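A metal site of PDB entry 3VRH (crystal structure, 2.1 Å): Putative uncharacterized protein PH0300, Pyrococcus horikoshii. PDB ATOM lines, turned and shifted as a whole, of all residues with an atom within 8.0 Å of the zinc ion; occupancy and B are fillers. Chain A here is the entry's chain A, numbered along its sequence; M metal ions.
The side-chain sulfur (SG) of Cys 3 lies close to the backbone NH (N) of Phe 5, 3.3 Å away.
The backbone NH (N) of Cys 3 is in hydrogen-bond range of the backbone carbonyl oxygen (O) of Arg 8, at 2.9 Å.
SG of Cys 22 lies close to N of Glu 24, 3.6 Å away.
N of Arg 8 sits close to SG of Cys 6.
Four residues have an atom within 4 Å of the zinc ion: Cys 3, Cys 6, Cys 22 and His 25.
A ring nitrogen (ND1) of His 25 binds the zinc ion.
SG of Cys 3 binds the zinc ion, at 2.4 Å.
The zinc ion is bound by SG of Cys 22, at 2.5 Å.
The side-chain sulfur (SG) of Cys 6 binds the zinc ion (2.5 Å).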
ATOM      1  N   LYS A   2     -12.733 -15.775 -19.621  1.00  0.00           N
ATOM      2  CA  LYS A   2     -11.452 -15.409 -19.020  1.00  0.00           C
ATOM      3  C   LYS A   2     -11.647 -14.991 -17.568  1.00  0.00           C
ATOM      4  O   LYS A   2     -12.738 -14.597 -17.163  1.00  0.00           O
ATOM      5  CB  LYS A   2     -10.758 -14.324 -19.834  1.00  0.00           C
ATOM      6  CG  LYS A   2     -10.288 -14.807 -21.217  1.00  0.00           C
ATOM      7  CD  LYS A   2      -9.368 -16.035 -21.110  1.00  0.00           C
ATOM      8  CE  LYS A   2      -9.192 -16.773 -22.450  1.00  0.00           C
ATOM      9  NZ  LYS A   2      -8.506 -18.104 -22.295  1.00  0.00           N
ATOM     10  N   CYS A   3     -10.570 -15.084 -16.797  1.00  0.00           N
ATOM     11  CA  CYS A   3     -10.620 -14.738 -15.397  1.00  0.00           C
ATOM     12  C   CYS A   3     -10.960 -13.259 -15.213  1.00  0.00           C
ATOM     13  O   CYS A   3     -10.607 -12.410 -16.032  1.00  0.00           O
ATOM     14  CB  CYS A   3      -9.276 -15.094 -14.731  1.00  0.00           C
ATOM     15  SG  CYS A   3      -9.161 -14.652 -12.984  1.00  0.00           S
ATOM     16  N   LYS A   4     -11.660 -12.962 -14.122  1.00  0.00           N
ATOM     17  CA  LYS A   4     -11.983 -11.590 -13.764  1.00  0.00           C
ATOM     18  C   LYS A   4     -10.728 -10.758 -13.466  1.00  0.00           C
ATOM     19  O   LYS A   4     -10.721  -9.546 -13.654  1.00  0.00           O
ATOM     20  CB  LYS A   4     -12.912 -11.567 -12.557  1.00  0.00           C
ATOM     21  CG  LYS A   4     -13.416 -10.175 -12.181  1.00  0.00           C
ATOM     22  CD  LYS A   4     -14.299 -10.180 -10.929  1.00  0.00           C
ATOM     23  CE  LYS A   4     -14.344  -8.801 -10.263  1.00  0.00           C
ATOM     24  NZ  LYS A   4     -15.205  -8.799  -9.028  1.00  0.00           N
ATOM     25  N   PHE A   5      -9.662 -11.419 -12.995  1.00  0.00           N
ATOM     26  CA  PHE A   5      -8.504 -10.707 -12.472  1.00  0.00           C
ATOM     27  C   PHE A   5      -7.240 -10.811 -13.318  1.00  0.00           C
ATOM     28  O   PHE A   5      -6.228 -10.164 -13.009  1.00  0.00           O
ATOM     29  CB  PHE A   5      -8.209 -11.150 -11.037  1.00  0.00           C
ATOM     30  CG  PHE A   5      -9.280 -10.767 -10.068  1.00  0.00           C
ATOM     31  CD1 PHE A   5      -9.390  -9.463  -9.614  1.00  0.00           C
ATOM     32  CD2 PHE A   5     -10.179 -11.710  -9.602  1.00  0.00           C
ATOM     33  CE1 PHE A   5     -10.396  -9.103  -8.716  1.00  0.00           C
ATOM     34  CE2 PHE A   5     -11.176 -11.359  -8.706  1.00  0.00           C
ATOM     35  CZ  PHE A   5     -11.284 -10.060  -8.265  1.00  0.00           C
ATOM     36  N   CYS A   6      -7.296 -11.611 -14.375  1.00  0.00           N
ATOM     37  CA  CYS A   6      -6.196 -11.723 -15.313  1.00  0.00           C
ATOM     38  C   CYS A   6      -6.683 -12.281 -16.636  1.00  0.00           C
ATOM     39  O   CYS A   6      -7.899 -12.385 -16.880  1.00  0.00           O
ATOM     40  CB  CYS A   6      -5.065 -12.591 -14.762  1.00  0.00           C
ATOM     41  SG  CYS A   6      -5.352 -14.385 -14.758  1.00  0.00           S
ATOM     42  N   SER A   7      -5.730 -12.642 -17.484  1.00  0.00           N
ATOM     43  CA  SER A   7      -5.992 -13.017 -18.865  1.00  0.00           C
ATOM     44  C   SER A   7      -6.045 -14.536 -19.031  1.00  0.00           C
ATOM     45  O   SER A   7      -6.246 -15.056 -20.142  1.00  0.00           O
ATOM     46  CB  SER A   7      -4.931 -12.370 -19.774  1.00  0.00           C
ATOM     47  OG  SER A   7      -4.669 -13.129 -20.932  1.00  0.00           O
ATOM     48  N   ARG A   8      -5.897 -15.265 -17.926  1.00  0.00           N
ATOM     49  CA  ARG A   8      -5.930 -16.726 -17.945  1.00  0.00           C
ATOM     50  C   ARG A   8      -7.340 -17.275 -18.154  1.00  0.00           C
ATOM     51  O   ARG A   8      -8.340 -16.593 -17.881  1.00  0.00           O
ATOM     52  CB  ARG A   8      -5.333 -17.314 -16.659  1.00  0.00           C
ATOM     53  CG  ARG A   8      -3.818 -17.102 -16.522  1.00  0.00           C
ATOM     54  CD  ARG A   8      -3.261 -17.718 -15.250  1.00  0.00           C
ATOM     55  NE  ARG A   8      -1.862 -17.348 -15.031  1.00  0.00           N
ATOM     56  CZ  ARG A   8      -1.459 -16.288 -14.328  1.00  0.00           C
ATOM     57  NH1 ARG A   8      -2.359 -15.487 -13.767  1.00  0.00           N
ATOM     58  NH2 ARG A   8      -0.155 -16.043 -14.181  1.00  0.00           N
ATOM     59  N   GLU A   9      -7.417 -18.505 -18.667  1.00  0.00           N
ATOM     60  CA  GLU A   9      -8.705 -19.155 -18.910  1.00  0.00           C
ATOM     61  C   GLU A   9      -9.453 -19.404 -17.589  1.00  0.00           C
ATOM     62  O   GLU A   9      -8.847 -19.760 -16.563  1.00  0.00           O
ATOM     63  CB  GLU A   9      -8.513 -20.468 -19.668  1.00  0.00           C
ATOM     64  CG  GLU A   9      -9.804 -21.005 -20.278  1.00  0.00           C
ATOM     65  CD  GLU A   9      -9.578 -22.178 -21.234  1.00  0.00           C
ATOM     66  OE1 GLU A   9      -8.525 -22.847 -21.128  1.00  0.00           O
ATOM     67  OE2 GLU A   9     -10.458 -22.419 -22.101  1.00  0.00           O
ATOM     68  N   ALA A  10     -10.764 -19.203 -17.610  1.00  0.00           N
ATOM     69  CA  ALA A  10     -11.583 -19.396 -16.423  1.00  0.00           C
ATOM     70  C   ALA A  10     -11.510 -20.848 -15.973  1.00  0.00           C
ATOM     71  O   ALA A  10     -11.554 -21.755 -16.780  1.00  0.00           O
ATOM     72  CB  ALA A  10     -13.014 -18.995 -16.717  1.00  0.00           C
ATOM     73  N   TYR A  11     -11.364 -21.061 -14.679  1.00  0.00           N
ATOM     74  CA  TYR A  11     -11.337 -22.419 -14.147  1.00  0.00           C
ATOM     75  C   TYR A  11     -12.683 -22.769 -13.568  1.00  0.00           C
ATOM     76  O   TYR A  11     -13.107 -23.931 -13.576  1.00  0.00           O
ATOM     77  CB  TYR A  11     -10.261 -22.530 -13.079  1.00  0.00           C
ATOM     78  CG  TYR A  11     -10.263 -23.827 -12.284  1.00  0.00           C
ATOM     79  CD1 TYR A  11      -9.971 -25.035 -12.902  1.00  0.00           C
ATOM     80  CD2 TYR A  11     -10.513 -23.822 -10.915  1.00  0.00           C
ATOM     81  CE1 TYR A  11      -9.937 -26.212 -12.183  1.00  0.00           C
ATOM     82  CE2 TYR A  11     -10.480 -25.006 -10.178  1.00  0.00           C
ATOM     83  CZ  TYR A  11     -10.186 -26.193 -10.819  1.00  0.00           C
ATOM     84  OH  TYR A  11     -10.150 -27.393 -10.121  1.00  0.00           O
ATOM     85  N   TYR A  20     -15.886 -15.121 -13.039  1.00  0.00           N
ATOM     86  CA  TYR A  20     -15.124 -16.261 -13.505  1.00  0.00           C
ATOM     87  C   TYR A  20     -13.730 -16.113 -12.945  1.00  0.00           C
ATOM     88  O   TYR A  20     -13.212 -14.992 -12.862  1.00  0.00           O
ATOM     89  CB  TYR A  20     -15.084 -16.305 -15.026  1.00  0.00           C
ATOM     90  CG  TYR A  20     -16.425 -16.621 -15.621  1.00  0.00           C
ATOM     91  CD1 TYR A  20     -16.792 -17.937 -15.876  1.00  0.00           C
ATOM     92  CD2 TYR A  20     -17.344 -15.614 -15.900  1.00  0.00           C
ATOM     93  CE1 TYR A  20     -18.027 -18.232 -16.410  1.00  0.00           C
ATOM     94  CE2 TYR A  20     -18.590 -15.909 -16.435  1.00  0.00           C
ATOM     95  CZ  TYR A  20     -18.927 -17.229 -16.678  1.00  0.00           C
ATOM     96  OH  TYR A  20     -20.162 -17.534 -17.217  1.00  0.00           O
ATOM     97  N   LEU A  21     -13.132 -17.231 -12.531  1.00  0.00           N
ATOM     98  CA  LEU A  21     -11.792 -17.228 -11.940  1.00  0.00           C
ATOM     99  C   LEU A  21     -10.921 -18.330 -12.512  1.00  0.00           C
ATOM    100  O   LEU A  21     -11.372 -19.458 -12.703  1.00  0.00           O
ATOM    101  CB  LEU A  21     -11.883 -17.403 -10.418  1.00  0.00           C
ATOM    102  CG  LEU A  21     -12.583 -16.349  -9.569  1.00  0.00           C
ATOM    103  CD1 LEU A  21     -12.560 -16.788  -8.109  1.00  0.00           C
ATOM    104  CD2 LEU A  21     -11.943 -14.967  -9.757  1.00  0.00           C
ATOM    105  N   CYS A  22      -9.649 -18.013 -12.762  1.00  0.00           N
ATOM    106  CA  CYS A  22      -8.672 -19.010 -13.140  1.00  0.00           C
ATOM    107  C   CYS A  22      -8.313 -19.832 -11.907  1.00  0.00           C
ATOM    108  O   CYS A  22      -8.744 -19.508 -10.785  1.00  0.00           O
ATOM    109  CB  CYS A  22      -7.407 -18.339 -13.686  1.00  0.00           C
ATOM    110  SG  CYS A  22      -6.373 -17.565 -12.426  1.00  0.00           S
ATOM    111  N   GLU A  23      -7.530 -20.889 -12.107  1.00  0.00           N
ATOM    112  CA  GLU A  23      -7.119 -21.774 -11.028  1.00  0.00           C
ATOM    113  C   GLU A  23      -6.511 -21.033  -9.846  1.00  0.00           C
ATOM    114  O   GLU A  23      -6.915 -21.246  -8.713  1.00  0.00           O
ATOM    115  CB  GLU A  23      -6.113 -22.802 -11.537  1.00  0.00           C
ATOM    116  CG  GLU A  23      -6.717 -23.981 -12.252  1.00  0.00           C
ATOM    117  CD  GLU A  23      -5.743 -25.148 -12.310  1.00  0.00           C
ATOM    118  OE1 GLU A  23      -5.858 -25.977 -13.253  1.00  0.00           O
ATOM    119  OE2 GLU A  23      -4.866 -25.232 -11.420  1.00  0.00           O
ATOM    120  N   GLU A  24      -5.536 -20.161 -10.119  1.00  0.00           N
ATOM    121  CA  GLU A  24      -4.791 -19.538  -9.033  1.00  0.00           C
ATOM    122  C   GLU A  24      -5.624 -18.511  -8.282  1.00  0.00           C
ATOM    123  O   GLU A  24      -5.532 -18.410  -7.064  1.00  0.00           O
ATOM    124  CB  GLU A  24      -3.498 -18.910  -9.551  1.00  0.00           C
ATOM    125  CG  GLU A  24      -2.433 -19.938  -9.903  1.00  0.00           C
ATOM    126  CD  GLU A  24      -2.050 -20.812  -8.723  1.00  0.00           C
ATOM    127  OE1 GLU A  24      -1.879 -20.274  -7.606  1.00  0.00           O
ATOM    128  OE2 GLU A  24      -1.931 -22.051  -8.898  1.00  0.00           O
ATOM    129  N   HIS A  25      -6.441 -17.764  -9.014  1.00  0.00           N
ATOM    130  CA  HIS A  25      -7.316 -16.785  -8.385  1.00  0.00           C
ATOM    131  C   HIS A  25      -8.482 -17.447  -7.676  1.00  0.00           C
ATOM    132  O   HIS A  25      -9.040 -16.864  -6.736  1.00  0.00           O
ATOM    133  CB  HIS A  25      -7.792 -15.710  -9.377  1.00  0.00           C
ATOM    134  CG  HIS A  25      -6.791 -14.623  -9.589  1.00  0.00           C
ATOM    135  ND1 HIS A  25      -6.122 -14.456 -10.776  1.00  0.00           N
ATOM    136  CD2 HIS A  25      -6.278 -13.700  -8.739  1.00  0.00           C
ATOM    137  CE1 HIS A  25      -5.274 -13.462 -10.679  1.00  0.00           C
ATOM    138  NE2 HIS A  25      -5.342 -12.977  -9.451  1.00  0.00           N
ATOM    139  N   PHE A  26      -8.865 -18.639  -8.119  1.00  0.00           N
ATOM    140  CA  PHE A  26      -9.864 -19.409  -7.378  1.00  0.00           C
ATOM    141  C   PHE A  26      -9.291 -19.881  -6.033  1.00  0.00           C
ATOM    142  O   PHE A  26      -9.957 -19.766  -4.996  1.00  0.00           O
ATOM    143  CB  PHE A  26     -10.352 -20.620  -8.163  1.00  0.00           C
ATOM    144  CG  PHE A  26     -11.147 -21.583  -7.338  1.00  0.00           C
ATOM    145  CD1 PHE A  26     -12.395 -21.213  -6.835  1.00  0.00           C
ATOM    146  CD2 PHE A  26     -10.641 -22.832  -7.030  1.00  0.00           C
ATOM    147  CE1 PHE A  26     -13.126 -22.089  -6.054  1.00  0.00           C
ATOM    148  CE2 PHE A  26     -11.372 -23.718  -6.253  1.00  0.00           C
ATOM    149  CZ  PHE A  26     -12.620 -23.344  -5.760  1.00  0.00           C
ATOM    150  N   GLU A  28      -6.945 -18.579  -4.318  1.00  0.00           N
ATOM    151  CA  GLU A  28      -6.880 -17.372  -3.500  1.00  0.00           C
ATOM    152  C   GLU A  28      -8.243 -16.975  -2.939  1.00  0.00           C
ATOM    153  O   GLU A  28      -8.369 -16.707  -1.742  1.00  0.00           O
ATOM    154  CB  GLU A  28      -6.285 -16.228  -4.328  1.00  0.00           C
ATOM    155  CG  GLU A  28      -6.273 -14.892  -3.611  1.00  0.00           C
ATOM    156  CD  GLU A  28      -5.454 -13.816  -4.343  1.00  0.00           C
ATOM    157  OE1 GLU A  28      -5.118 -13.995  -5.530  1.00  0.00           O
ATOM    158  OE2 GLU A  28      -5.157 -12.777  -3.700  1.00  0.00           O
HETATM  159 ZN    ZN M   1      -6.789 -15.107 -12.807  1.00  0.00          ZN
